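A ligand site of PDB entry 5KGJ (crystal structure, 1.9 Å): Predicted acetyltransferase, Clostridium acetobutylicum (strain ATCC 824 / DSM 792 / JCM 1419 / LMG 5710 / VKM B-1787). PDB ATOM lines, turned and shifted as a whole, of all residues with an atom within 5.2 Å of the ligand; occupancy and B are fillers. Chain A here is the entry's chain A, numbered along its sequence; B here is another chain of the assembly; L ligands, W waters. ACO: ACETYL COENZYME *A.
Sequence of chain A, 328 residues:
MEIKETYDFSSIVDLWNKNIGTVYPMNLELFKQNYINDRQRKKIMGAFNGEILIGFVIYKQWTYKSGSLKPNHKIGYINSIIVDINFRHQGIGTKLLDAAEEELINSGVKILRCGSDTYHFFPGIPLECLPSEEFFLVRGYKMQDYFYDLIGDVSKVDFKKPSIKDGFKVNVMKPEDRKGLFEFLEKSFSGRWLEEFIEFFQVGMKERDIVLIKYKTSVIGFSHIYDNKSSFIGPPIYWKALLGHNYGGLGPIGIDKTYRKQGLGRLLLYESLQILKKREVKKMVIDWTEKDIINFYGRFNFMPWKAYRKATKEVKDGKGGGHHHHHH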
ATOM      1  N   ILE A  20     -24.101 -33.723 -23.097  1.00  0.00           N
ATOM      2  CA  ILE A  20     -25.120 -34.438 -22.351  1.00  0.00           C
ATOM      3  C   ILE A  20     -25.667 -35.700 -23.015  1.00  0.00           C
ATOM      4  O   ILE A  20     -26.644 -36.282 -22.540  1.00  0.00           O
ATOM      5  CB  ILE A  20     -26.276 -33.511 -21.918  1.00  0.00           C
ATOM      6  CG1 ILE A  20     -27.214 -33.149 -23.090  1.00  0.00           C
ATOM      7  CG2 ILE A  20     -25.747 -32.307 -21.172  1.00  0.00           C
ATOM      8  CD1 ILE A  20     -28.404 -32.285 -22.688  1.00  0.00           C
ATOM      9  N   ILE A  78     -37.733 -21.466 -22.241  1.00  0.00           N
ATOM     10  CA  ILE A  78     -36.378 -21.878 -22.560  1.00  0.00           C
ATOM     11  C   ILE A  78     -36.451 -23.376 -22.845  1.00  0.00           C
ATOM     12  O   ILE A  78     -36.693 -24.159 -21.916  1.00  0.00           O
ATOM     13  CB  ILE A  78     -35.427 -21.617 -21.378  1.00  0.00           C
ATOM     14  CG1 ILE A  78     -35.630 -20.186 -20.872  1.00  0.00           C
ATOM     15  CG2 ILE A  78     -33.998 -21.927 -21.777  1.00  0.00           C
ATOM     16  CD1 ILE A  78     -35.383 -19.135 -21.925  1.00  0.00           C
ATOM     17  N   ASN A  79     -36.371 -23.728 -24.125  1.00  0.00           N
ATOM     18  CA  ASN A  79     -36.508 -25.085 -24.597  1.00  0.00           C
ATOM     19  C   ASN A  79     -35.281 -25.895 -24.147  1.00  0.00           C
ATOM     20  O   ASN A  79     -35.404 -27.024 -23.662  1.00  0.00           O
ATOM     21  CB  ASN A  79     -36.643 -25.078 -26.120  1.00  0.00           C
ATOM     22  CG  ASN A  79     -36.323 -26.423 -26.756  1.00  0.00           C
ATOM     23  OD1 ASN A  79     -35.155 -26.733 -27.023  1.00  0.00           O
ATOM     24  ND2 ASN A  79     -37.355 -27.179 -27.094  1.00  0.00           N
ATOM     25  N   SER A  80     -34.118 -25.301 -24.330  1.00  0.00           N
ATOM     26  CA  SER A  80     -32.853 -25.870 -23.927  1.00  0.00           C
ATOM     27  C   SER A  80     -31.782 -24.744 -23.906  1.00  0.00           C
ATOM     28  O   SER A  80     -31.895 -23.710 -24.596  1.00  0.00           O
ATOM     29  CB  SER A  80     -32.440 -26.976 -24.899  1.00  0.00           C
ATOM     30  OG  SER A  80     -32.571 -26.585 -26.258  1.00  0.00           O
ATOM     31  N   ILE A  81     -30.765 -24.975 -23.096  1.00  0.00           N
ATOM     32  CA  ILE A  81     -29.539 -24.181 -23.143  1.00  0.00           C
ATOM     33  C   ILE A  81     -28.344 -25.038 -22.710  1.00  0.00           C
ATOM     34  O   ILE A  81     -28.408 -25.712 -21.697  1.00  0.00           O
ATOM     35  CB  ILE A  81     -29.664 -22.953 -22.227  1.00  0.00           C
ATOM     36  CG1 ILE A  81     -28.354 -22.150 -22.216  1.00  0.00           C
ATOM     37  CG2 ILE A  81     -30.060 -23.324 -20.802  1.00  0.00           C
ATOM     38  CD1 ILE A  81     -28.557 -20.796 -21.550  1.00  0.00           C
ATOM     39  N   ILE A  82     -27.302 -25.061 -23.520  1.00  0.00           N
ATOM     40  CA  ILE A  82     -26.104 -25.826 -23.203  1.00  0.00           C
ATOM     41  C   ILE A  82     -24.917 -24.952 -23.622  1.00  0.00           C
ATOM     42  O   ILE A  82     -24.890 -24.442 -24.749  1.00  0.00           O
ATOM     43  CB  ILE A  82     -26.006 -27.143 -23.975  1.00  0.00           C
ATOM     44  CG1 ILE A  82     -27.302 -27.983 -23.838  1.00  0.00           C
ATOM     45  CG2 ILE A  82     -24.741 -27.894 -23.544  1.00  0.00           C
ATOM     46  CD1 ILE A  82     -27.298 -29.266 -24.638  1.00  0.00           C
ATOM     47  N   VAL A  83     -23.970 -24.779 -22.699  1.00  0.00           N
ATOM     48  CA  VAL A  83     -22.611 -24.282 -22.961  1.00  0.00           C
ATOM     49  C   VAL A  83     -21.616 -25.407 -22.958  1.00  0.00           C
ATOM     50  O   VAL A  83     -21.647 -26.321 -22.074  1.00  0.00           O
ATOM     51  CB  VAL A  83     -22.267 -23.221 -21.904  1.00  0.00           C
ATOM     52  CG1 VAL A  83     -20.776 -22.825 -21.928  1.00  0.00           C
ATOM     53  CG2 VAL A  83     -23.180 -22.001 -22.115  1.00  0.00           C
ATOM     54  N   PHE A  87     -15.892 -24.422 -21.919  1.00  0.00           N
ATOM     55  CA  PHE A  87     -16.108 -22.982 -21.866  1.00  0.00           C
ATOM     56  C   PHE A  87     -17.024 -22.511 -20.754  1.00  0.00           C
ATOM     57  O   PHE A  87     -17.639 -21.472 -20.834  1.00  0.00           O
ATOM     58  CB  PHE A  87     -16.607 -22.521 -23.241  1.00  0.00           C
ATOM     59  CG  PHE A  87     -15.616 -22.805 -24.351  1.00  0.00           C
ATOM     60  CD1 PHE A  87     -14.655 -21.840 -24.713  1.00  0.00           C
ATOM     61  CD2 PHE A  87     -15.616 -24.000 -25.006  1.00  0.00           C
ATOM     62  CE1 PHE A  87     -13.729 -22.088 -25.717  1.00  0.00           C
ATOM     63  CE2 PHE A  87     -14.693 -24.266 -25.997  1.00  0.00           C
ATOM     64  CZ  PHE A  87     -13.756 -23.297 -26.373  1.00  0.00           C
ATOM     65  N   ARG A  88     -17.096 -23.287 -19.674  1.00  0.00           N
ATOM     66  CA  ARG A  88     -18.050 -23.031 -18.592  1.00  0.00           C
ATOM     67  C   ARG A  88     -17.524 -21.970 -17.632  1.00  0.00           C
ATOM     68  O   ARG A  88     -16.330 -21.701 -17.572  1.00  0.00           O
ATOM     69  CB  ARG A  88     -18.248 -24.304 -17.745  1.00  0.00           C
ATOM     70  CG  ARG A  88     -18.862 -25.495 -18.471  1.00  0.00           C
ATOM     71  CD  ARG A  88     -20.377 -25.360 -18.611  1.00  0.00           C
ATOM     72  NE  ARG A  88     -20.875 -26.417 -19.492  1.00  0.00           N
ATOM     73  CZ  ARG A  88     -21.124 -27.667 -19.155  1.00  0.00           C
ATOM     74  NH1 ARG A  88     -21.531 -28.518 -20.098  1.00  0.00           N
ATOM     75  NH2 ARG A  88     -21.006 -28.092 -17.910  1.00  0.00           N
ATOM     76  N   HIS A  89     -18.424 -21.377 -16.862  1.00  0.00           N
ATOM     77  CA  HIS A  89     -18.065 -20.385 -15.892  1.00  0.00           C
ATOM     78  C   HIS A  89     -17.245 -19.276 -16.505  1.00  0.00           C
ATOM     79  O   HIS A  89     -16.341 -18.775 -15.874  1.00  0.00           O
ATOM     80  CB  HIS A  89     -17.328 -20.999 -14.669  1.00  0.00           C
ATOM     81  CG  HIS A  89     -18.206 -21.867 -13.829  1.00  0.00           C
ATOM     82  ND1 HIS A  89     -19.091 -21.359 -12.913  1.00  0.00           N
ATOM     83  CD2 HIS A  89     -18.377 -23.210 -13.805  1.00  0.00           C
ATOM     84  CE1 HIS A  89     -19.735 -22.347 -12.322  1.00  0.00           C
ATOM     85  NE2 HIS A  89     -19.315 -23.472 -12.849  1.00  0.00           N
ATOM     86  N   GLN A  90     -17.607 -18.855 -17.717  1.00  0.00           N
ATOM     87  CA  GLN A  90     -17.056 -17.637 -18.279  1.00  0.00           C
ATOM     88  C   GLN A  90     -18.141 -16.625 -18.627  1.00  0.00           C
ATOM     89  O   GLN A  90     -17.841 -15.678 -19.337  1.00  0.00           O
ATOM     90  CB  GLN A  90     -16.270 -17.946 -19.556  1.00  0.00           C
ATOM     91  CG  GLN A  90     -15.214 -19.020 -19.444  1.00  0.00           C
ATOM     92  CD  GLN A  90     -14.504 -19.176 -20.758  1.00  0.00           C
ATOM     93  OE1 GLN A  90     -14.678 -18.387 -21.671  1.00  0.00           O
ATOM     94  NE2 GLN A  90     -13.723 -20.245 -20.882  1.00  0.00           N
ATOM     95  N   GLY A  91     -19.373 -16.828 -18.154  1.00  0.00           N
ATOM     96  CA  GLY A  91     -20.466 -15.919 -18.379  1.00  0.00           C
ATOM     97  C   GLY A  91     -21.214 -16.154 -19.671  1.00  0.00           C
ATOM     98  O   GLY A  91     -22.122 -15.386 -20.012  1.00  0.00           O
ATOM     99  N   ILE A  92     -20.860 -17.203 -20.401  1.00  0.00           N
ATOM    100  CA  ILE A  92     -21.485 -17.416 -21.683  1.00  0.00           C
ATOM    101  C   ILE A  92     -22.947 -17.808 -21.581  1.00  0.00           C
ATOM    102  O   ILE A  92     -23.790 -17.280 -22.313  1.00  0.00           O
ATOM    103  CB  ILE A  92     -20.738 -18.440 -22.507  1.00  0.00           C
ATOM    104  CG1 ILE A  92     -19.331 -17.902 -22.810  1.00  0.00           C
ATOM    105  CG2 ILE A  92     -21.538 -18.797 -23.762  1.00  0.00           C
ATOM    106  CD1 ILE A  92     -18.418 -18.960 -23.420  1.00  0.00           C
ATOM    107  N   GLY A  93     -23.241 -18.713 -20.657  1.00  0.00           N
ATOM    108  CA  GLY A  93     -24.621 -19.055 -20.354  1.00  0.00           C
ATOM    109  C   GLY A  93     -25.489 -17.871 -20.006  1.00  0.00           C
ATOM    110  O   GLY A  93     -26.624 -17.717 -20.502  1.00  0.00           O
ATOM    111  N   THR A  94     -24.945 -17.020 -19.125  1.00  0.00           N
ATOM    112  CA  THR A  94     -25.529 -15.733 -18.806  1.00  0.00           C
ATOM    113  C   THR A  94     -25.876 -14.847 -20.000  1.00  0.00           C
ATOM    114  O   THR A  94     -27.034 -14.401 -20.116  1.00  0.00           O
ATOM    115  CB  THR A  94     -24.662 -14.955 -17.803  1.00  0.00           C
ATOM    116  OG1 THR A  94     -24.512 -15.733 -16.621  1.00  0.00           O
ATOM    117  CG2 THR A  94     -25.359 -13.600 -17.412  1.00  0.00           C
ATOM    118  N   CYS A 114     -38.892 -23.186 -17.792  1.00  0.00           N
ATOM    119  CA  CYS A 114     -37.825 -24.073 -18.161  1.00  0.00           C
ATOM    120  C   CYS A 114     -38.461 -25.296 -18.733  1.00  0.00           C
ATOM    121  O   CYS A 114     -39.120 -26.059 -18.034  1.00  0.00           O
ATOM    122  CB  CYS A 114     -36.955 -24.415 -16.940  1.00  0.00           C
ATOM    123  SG  CYS A 114     -35.862 -23.049 -16.421  1.00  0.00           S
ATOM    124  N   GLY A 115     -38.217 -25.527 -20.013  1.00  0.00           N
ATOM    125  CA  GLY A 115     -38.870 -26.572 -20.740  1.00  0.00           C
ATOM    126  C   GLY A 115     -40.394 -26.456 -20.661  1.00  0.00           C
ATOM    127  O   GLY A 115     -40.950 -25.346 -20.540  1.00  0.00           O
ATOM    128  N   PHE A 122     -37.664 -31.315 -22.857  1.00  0.00           N
ATOM    129  CA  PHE A 122     -37.658 -31.549 -21.422  1.00  0.00           C
ATOM    130  C   PHE A 122     -38.936 -30.998 -20.785  1.00  0.00           C
ATOM    131  O   PHE A 122     -39.283 -29.859 -21.021  1.00  0.00           O
ATOM    132  CB  PHE A 122     -36.521 -30.823 -20.751  1.00  0.00           C
ATOM    133  CG  PHE A 122     -35.157 -31.081 -21.318  1.00  0.00           C
ATOM    134  CD1 PHE A 122     -34.605 -32.346 -21.340  1.00  0.00           C
ATOM    135  CD2 PHE A 122     -34.387 -30.019 -21.749  1.00  0.00           C
ATOM    136  CE1 PHE A 122     -33.331 -32.564 -21.843  1.00  0.00           C
ATOM    137  CE2 PHE A 122     -33.077 -30.220 -22.209  1.00  0.00           C
ATOM    138  CZ  PHE A 122     -32.567 -31.489 -22.274  1.00  0.00           C
ATOM    139  N   GLY A 124     -39.098 -30.231 -17.743  1.00  0.00           N
ATOM    140  CA  GLY A 124     -38.494 -29.256 -16.827  1.00  0.00           C
ATOM    141  C   GLY A 124     -36.968 -29.430 -16.774  1.00  0.00           C
ATOM    142  O   GLY A 124     -36.371 -30.036 -17.668  1.00  0.00           O
ATOM    143  N   ILE A 125     -36.340 -28.915 -15.728  1.00  0.00           N
ATOM    144  CA  ILE A 125     -34.891 -29.075 -15.569  1.00  0.00           C
ATOM    145  C   ILE A 125     -34.570 -30.508 -15.210  1.00  0.00           C
ATOM    146  O   ILE A 125     -34.950 -30.977 -14.164  1.00  0.00           O
ATOM    147  CB  ILE A 125     -34.336 -28.170 -14.480  1.00  0.00           C
ATOM    148  CG1 ILE A 125     -34.719 -26.707 -14.795  1.00  0.00           C
ATOM    149  CG2 ILE A 125     -32.826 -28.314 -14.376  1.00  0.00           C
ATOM    150  CD1 ILE A 125     -34.334 -25.754 -13.671  1.00  0.00           C
ATOM    151  N   PRO A 126     -33.904 -31.229 -16.115  1.00  0.00           N
ATOM    152  CA  PRO A 126     -33.583 -32.614 -15.769  1.00  0.00           C
ATOM    153  C   PRO A 126     -32.757 -32.758 -14.484  1.00  0.00           C
ATOM    154  O   PRO A 126     -31.886 -31.946 -14.195  1.00  0.00           O
ATOM    155  CB  PRO A 126     -32.759 -33.096 -16.967  1.00  0.00           C
ATOM    156  CG  PRO A 126     -33.144 -32.207 -18.083  1.00  0.00           C
ATOM    157  CD  PRO A 126     -33.364 -30.884 -17.440  1.00  0.00           C
ATOM    158  N   CYS A 129     -29.239 -32.569 -14.974  1.00  0.00           N
ATOM    159  CA  CYS A 129     -28.813 -31.154 -15.027  1.00  0.00           C
ATOM    160  C   CYS A 129     -29.107 -30.418 -13.749  1.00  0.00           C
ATOM    161  O   CYS A 129     -29.263 -29.184 -13.731  1.00  0.00           O
ATOM    162  CB  CYS A 129     -29.555 -30.466 -16.162  1.00  0.00           C
ATOM    163  SG  CYS A 129     -29.221 -31.218 -17.780  1.00  0.00           S
ATOM    164  N   PRO A 131     -27.265 -29.374 -11.338  1.00  0.00           N
ATOM    165  CA  PRO A 131     -26.446 -28.236 -10.944  1.00  0.00           C
ATOM    166  C   PRO A 131     -26.867 -26.921 -11.620  1.00  0.00           C
ATOM    167  O   PRO A 131     -26.570 -25.866 -11.087  1.00  0.00           O
ATOM    168  CB  PRO A 131     -25.029 -28.653 -11.383  1.00  0.00           C
ATOM    169  CG  PRO A 131     -25.053 -30.161 -11.307  1.00  0.00           C
ATOM    170  CD  PRO A 131     -26.435 -30.493 -11.839  1.00  0.00           C
ATOM    171  N   SER A 132     -27.505 -27.003 -12.798  1.00  0.00           N
ATOM    172  CA  SER A 132     -28.067 -25.853 -13.482  1.00  0.00           C
ATOM    173  C   SER A 132     -29.215 -25.234 -12.707  1.00  0.00           C
ATOM    174  O   SER A 132     -29.532 -24.064 -12.955  1.00  0.00           O
ATOM    175  CB  SER A 132     -28.563 -26.228 -14.889  1.00  0.00           C
ATOM    176  OG  SER A 132     -29.813 -26.884 -14.858  1.00  0.00           O
ATOM    177  N   GLU A 134     -29.079 -24.041  -9.913  1.00  0.00           N
ATOM    178  CA  GLU A 134     -28.462 -22.893  -9.288  1.00  0.00           C
ATOM    179  C   GLU A 134     -28.173 -21.752 -10.259  1.00  0.00           C
ATOM    180  O   GLU A 134     -28.242 -20.557  -9.924  1.00  0.00           O
ATOM    181  CB  GLU A 134     -27.179 -23.383  -8.599  1.00  0.00           C
ATOM    182  CG  GLU A 134     -26.581 -22.421  -7.634  1.00  0.00           C
ATOM    183  CD  GLU A 134     -27.535 -22.168  -6.482  1.00  0.00           C
ATOM    184  OE1 GLU A 134     -28.208 -23.136  -6.004  1.00  0.00           O
ATOM    185  OE2 GLU A 134     -27.593 -20.976  -6.097  1.00  0.00           O
ATOM    186  N   PHE A 135     -27.779 -22.109 -11.479  1.00  0.00           N
ATOM    187  CA  PHE A 135     -27.729 -21.154 -12.566  1.00  0.00           C
ATOM    188  C   PHE A 135     -29.072 -20.443 -12.738  1.00  0.00           C
ATOM    189  O   PHE A 135     -29.096 -19.217 -12.875  1.00  0.00           O
ATOM    190  CB  PHE A 135     -27.309 -21.851 -13.863  1.00  0.00           C
ATOM    191  CG  PHE A 135     -27.408 -21.013 -15.112  1.00  0.00           C
ATOM    192  CD1 PHE A 135     -26.407 -20.085 -15.425  1.00  0.00           C
ATOM    193  CD2 PHE A 135     -28.426 -21.222 -16.009  1.00  0.00           C
ATOM    194  CE1 PHE A 135     -26.483 -19.365 -16.594  1.00  0.00           C
ATOM    195  CE2 PHE A 135     -28.499 -20.508 -17.200  1.00  0.00           C
ATOM    196  CZ  PHE A 135     -27.514 -19.572 -17.499  1.00  0.00           C
ATOM    197  N   PHE A 136     -30.163 -21.192 -12.724  1.00  0.00           N
ATOM    198  CA  PHE A 136     -31.484 -20.610 -12.971  1.00  0.00           C
ATOM    199  C   PHE A 136     -31.957 -19.802 -11.763  1.00  0.00           C
ATOM    200  O   PHE A 136     -32.417 -18.644 -11.900  1.00  0.00           O
ATOM    201  CB  PHE A 136     -32.515 -21.678 -13.407  1.00  0.00           C
ATOM    202  CG  PHE A 136     -32.302 -22.197 -14.818  1.00  0.00           C
ATOM    203  CD1 PHE A 136     -32.586 -21.402 -15.909  1.00  0.00           C
ATOM    204  CD2 PHE A 136     -31.811 -23.486 -15.040  1.00  0.00           C
ATOM    205  CE1 PHE A 136     -32.373 -21.862 -17.191  1.00  0.00           C
ATOM    206  CE2 PHE A 136     -31.586 -23.949 -16.315  1.00  0.00           C
ATOM    207  CZ  PHE A 136     -31.879 -23.158 -17.391  1.00  0.00           C
ATOM    208  N   VAL A 138     -30.082 -18.181  -9.598  1.00  0.00           N
ATOM    209  CA  VAL A 138     -29.387 -16.924  -9.633  1.00  0.00           C
ATOM    210  C   VAL A 138     -30.066 -15.927 -10.586  1.00  0.00           C
ATOM    211  O   VAL A 138     -30.028 -14.739 -10.334  1.00  0.00           O
ATOM    212  CB  VAL A 138     -27.918 -17.136 -10.013  1.00  0.00           C
ATOM    213  CG1 VAL A 138     -27.283 -15.824 -10.465  1.00  0.00           C
ATOM    214  CG2 VAL A 138     -27.154 -17.735  -8.832  1.00  0.00           C
ATOM    215  N   ASN B 295     -20.334 -30.640  -8.398  1.00  0.00           N
ATOM    216  CA  ASN B 295     -19.592 -29.719  -9.302  1.00  0.00           C
ATOM    217  C   ASN B 295     -18.111 -30.058  -9.475  1.00  0.00           C
ATOM    218  O   ASN B 295     -17.506 -29.793 -10.526  1.00  0.00           O
ATOM    219  CB  ASN B 295     -19.749 -28.263  -8.837  1.00  0.00           C
ATOM    220  CG  ASN B 295     -21.063 -27.640  -9.252  1.00  0.00           C
ATOM    221  OD1 ASN B 295     -21.502 -26.612  -8.694  1.00  0.00           O
ATOM    222  ND2 ASN B 295     -21.714 -28.248 -10.218  1.00  0.00           N
HETATM  223  N1A ACO L   1     -23.343 -24.808  -9.983  1.00  0.00           N
HETATM  224  C2A ACO L   1     -23.707 -23.742  -9.231  1.00  0.00           C
HETATM  225  N3A ACO L   1     -23.897 -22.537  -9.795  1.00  0.00           N
HETATM  226  C4A ACO L   1     -23.709 -22.383 -11.131  1.00  0.00           C
HETATM  227  C5A ACO L   1     -23.316 -23.502 -12.005  1.00  0.00           C
HETATM  228  C6A ACO L   1     -23.128 -24.775 -11.330  1.00  0.00           C
HETATM  229  N6A ACO L   1     -22.764 -25.816 -12.131  1.00  0.00           N
HETATM  230  N7A ACO L   1     -23.201 -23.071 -13.261  1.00  0.00           N
HETATM  231  C8A ACO L   1     -23.479 -21.749 -13.234  1.00  0.00           C
HETATM  232  N9A ACO L   1     -23.814 -21.356 -11.977  1.00  0.00           N
HETATM  233  C1B ACO L   1     -24.189 -20.002 -11.497  1.00  0.00           C
HETATM  234  C2B ACO L   1     -22.938 -19.367 -10.878  1.00  0.00           C
HETATM  235  O2B ACO L   1     -23.353 -18.413  -9.904  1.00  0.00           O
HETATM  236  C3B ACO L   1     -22.295 -18.699 -12.068  1.00  0.00           C
HETATM  237  O3B ACO L   1     -21.393 -17.687 -11.644  1.00  0.00           O
HETATM  238  P3B ACO L   1     -19.867 -18.039 -11.222  1.00  0.00           P
HETATM  239  O7A ACO L   1     -19.171 -18.600 -12.439  1.00  0.00           O
HETATM  240  O8A ACO L   1     -19.429 -16.633 -10.794  1.00  0.00           O
HETATM  241  O9A ACO L   1     -19.987 -19.013 -10.108  1.00  0.00           O
HETATM  242  C4B ACO L   1     -23.547 -18.224 -12.815  1.00  0.00           C
HETATM  243  O4B ACO L   1     -24.538 -19.253 -12.647  1.00  0.00           O
HETATM  244  C5B ACO L   1     -23.343 -17.892 -14.278  1.00  0.00           C
HETATM  245  O5B ACO L   1     -22.718 -18.949 -14.963  1.00  0.00           O
HETATM  246  P1A ACO L   1     -22.259 -18.813 -16.453  1.00  0.00           P
HETATM  247  O1A ACO L   1     -20.756 -18.820 -16.521  1.00  0.00           O
HETATM  248  O2A ACO L   1     -23.034 -17.647 -17.011  1.00  0.00           O
HETATM  249  O3A ACO L   1     -22.823 -20.282 -16.871  1.00  0.00           O
HETATM  250  P2A ACO L   1     -22.177 -21.220 -17.975  1.00  0.00           P
HETATM  251  O4A ACO L   1     -21.679 -20.504 -19.201  1.00  0.00           O
HETATM  252  O5A ACO L   1     -21.246 -22.146 -17.271  1.00  0.00           O
HETATM  253  O6A ACO L   1     -23.502 -22.057 -18.377  1.00  0.00           O
HETATM  254  CBP ACO L   1     -25.032 -23.946 -17.994  1.00  0.00           C
HETATM  255  CCP ACO L   1     -24.412 -22.668 -17.435  1.00  0.00           C
HETATM  256  CDP ACO L   1     -25.691 -23.551 -19.331  1.00  0.00           C
HETATM  257  CEP ACO L   1     -26.063 -24.454 -16.985  1.00  0.00           C
HETATM  258  CAP ACO L   1     -23.922 -24.999 -18.178  1.00  0.00           C
HETATM  259  OAP ACO L   1     -23.425 -25.427 -16.886  1.00  0.00           O
HETATM  260  C9P ACO L   1     -24.387 -26.168 -19.007  1.00  0.00           C
HETATM  261  O9P ACO L   1     -24.463 -26.141 -20.245  1.00  0.00           O
HETATM  262  N8P ACO L   1     -24.705 -27.236 -18.288  1.00  0.00           N
HETATM  263  C7P ACO L   1     -25.121 -28.450 -18.920  1.00  0.00           C
HETATM  264  C6P ACO L   1     -26.485 -28.317 -19.596  1.00  0.00           C
HETATM  265  C5P ACO L   1     -27.591 -27.903 -18.673  1.00  0.00           C
HETATM  266  O5P ACO L   1     -27.605 -28.351 -17.508  1.00  0.00           O
HETATM  267  N4P ACO L   1     -28.533 -27.097 -19.225  1.00  0.00           N
HETATM  268  C3P ACO L   1     -29.759 -26.719 -18.546  1.00  0.00           C
HETATM  269  C2P ACO L   1     -30.834 -27.801 -18.756  1.00  0.00           C
HETATM  270  S1P ACO L   1     -32.484 -27.292 -18.401  1.00  0.00           S
HETATM  271  C   ACO L   1     -32.992 -26.433 -19.768  1.00  0.00           C
HETATM  272  O   ACO L   1     -32.271 -26.317 -20.739  1.00  0.00           O
HETATM  273  CH3 ACO L   1     -34.391 -25.864 -19.804  1.00  0.00           C
HETATM  274  O   HOH W   1     -23.427 -14.561 -14.214  1.00  0.00           O
HETATM  275  O   HOH W   2     -19.546 -25.717 -11.552  1.00  0.00           O
HETATM  276  O   HOH W   3     -17.803 -15.094 -12.273  1.00  0.00           O
HETATM  277  O   HOH W   4     -21.719 -23.959 -15.479  1.00  0.00           O
HETATM  278  O   HOH W   5     -24.224 -27.254 -14.787  1.00  0.00           O
HETATM  279  O   HOH W   6     -26.098 -29.132 -15.391  1.00  0.00           O
HETATM  280  O   HOH W   7     -27.074 -17.592 -13.369  1.00  0.00           O
HETATM  281  O   HOH W   8     -17.561 -16.022  -8.782  1.00  0.00           O
HETATM  282  O   HOH W   9     -19.458 -17.230 -14.710  1.00  0.00           O
HETATM  283  O   HOH W  10     -21.673 -15.995  -9.904  1.00  0.00           O
HETATM  284  O   HOH W  11     -16.530 -18.097 -12.700  1.00  0.00           O
HETATM  285  O   HOH W  12     -24.133 -19.810  -8.099  1.00  0.00           O
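The guanidinium group (NE) of Arg 88 is in hydrogen-bond range of the backbone carbonyl oxygen (O) of Val 83 (2.7 Å).
The side-chain hydroxyl (OG) of Ser 132 is in hydrogen-bond range of the backbone carbonyl oxygen (O) of Cys 129 (2.6 Å).
The side-chain hydroxyl (OG) of Ser 80 lies within hydrogen-bond range of the side-chain amide oxygen (OD1) of Asn 79.
The backbone NH of Gly 115 lies within hydrogen-bond range of the backbone carbonyl oxygen of Ile 78 (2.8 Å).
Water W9 bridges an oxygen (O7A) of the ligand (2.7 Å) and the backbone NH of Gly 91 (3.5 Å).
Water W11 bridges an oxygen (O7A) of the ligand and the backbone carbonyl oxygen (O) of His 89.
Water W7 bridges O of Phe 135 and O4B of the ligand.
Water W2 lies within hydrogen-bond range of NE2 of His 89 (2.6 Å) and N6A of the ligand (3.3 Å).
The backbone NH (N) of Thr 94 lies within hydrogen-bond range of an oxygen (O2A) of the ligand, at 2.9 Å.
The side-chain hydroxyl (OG1) of Thr 94 sits at hydrogen-bond distance from an oxygen (O2A) of the ligand (2.4 Å).
The backbone NH of Gly 93 sits at hydrogen-bond distance from an oxygen (O4A) of the ligand.
An oxygen (O5A) of the ligand sits at hydrogen-bond distance from the backbone NH (N) of His 89.
ND1 of His 89 is in hydrogen-bond range of O7A of the ligand.
O of the ligand sits at hydrogen-bond distance from N of Ile 81 (3.1 Å).
O of Ile 81 lies within hydrogen-bond range of N4P of the ligand, 2.8 Å away.
An oxygen (O9P) of the ligand lies within hydrogen-bond range of the backbone NH of Val 83 (2.8 Å).
OD1 of Asn 295 of chain B sits close to N1A of the ligand (2.9 Å).
The backbone NH (N) of Gly 91 lies within hydrogen-bond range of an oxygen (O1A) of the ligand, 2.9 Å away.
SG of Cys 129 lies close to O5P of the ligand, at 3.3 Å.
N of Gln 90 is in hydrogen-bond range of O1A of the ligand.
Merely in contact with the ligand: Ser 80, Ile 82, Glu 134, Phe 135, Arg 88, Ser 132, Ile 78, Pro 131, Ile 92, Pro 126, Gly 115 and Phe 136.
Hydrophobic or aromatic side chains that line the ligand: Ile 81, Ile 82, Val 83, His 89, Pro 126, Pro 131, Phe 135 and Phe 136.
Within 4 Å of the ligand: Ile 78, Ser 80, Ile 81, Ile 82, Val 83, Arg 88, His 89, Gln 90, Gly 91, Ile 92, Gly 93, Thr 94, Gly 115, Pro 126, Cys 129, Pro 131, Ser 132, Glu 134, Phe 135, Phe 136 and Asn 295 of chain B.
The nearest printed residue that does not touch the ligand is Val 138 (4.01 Å).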
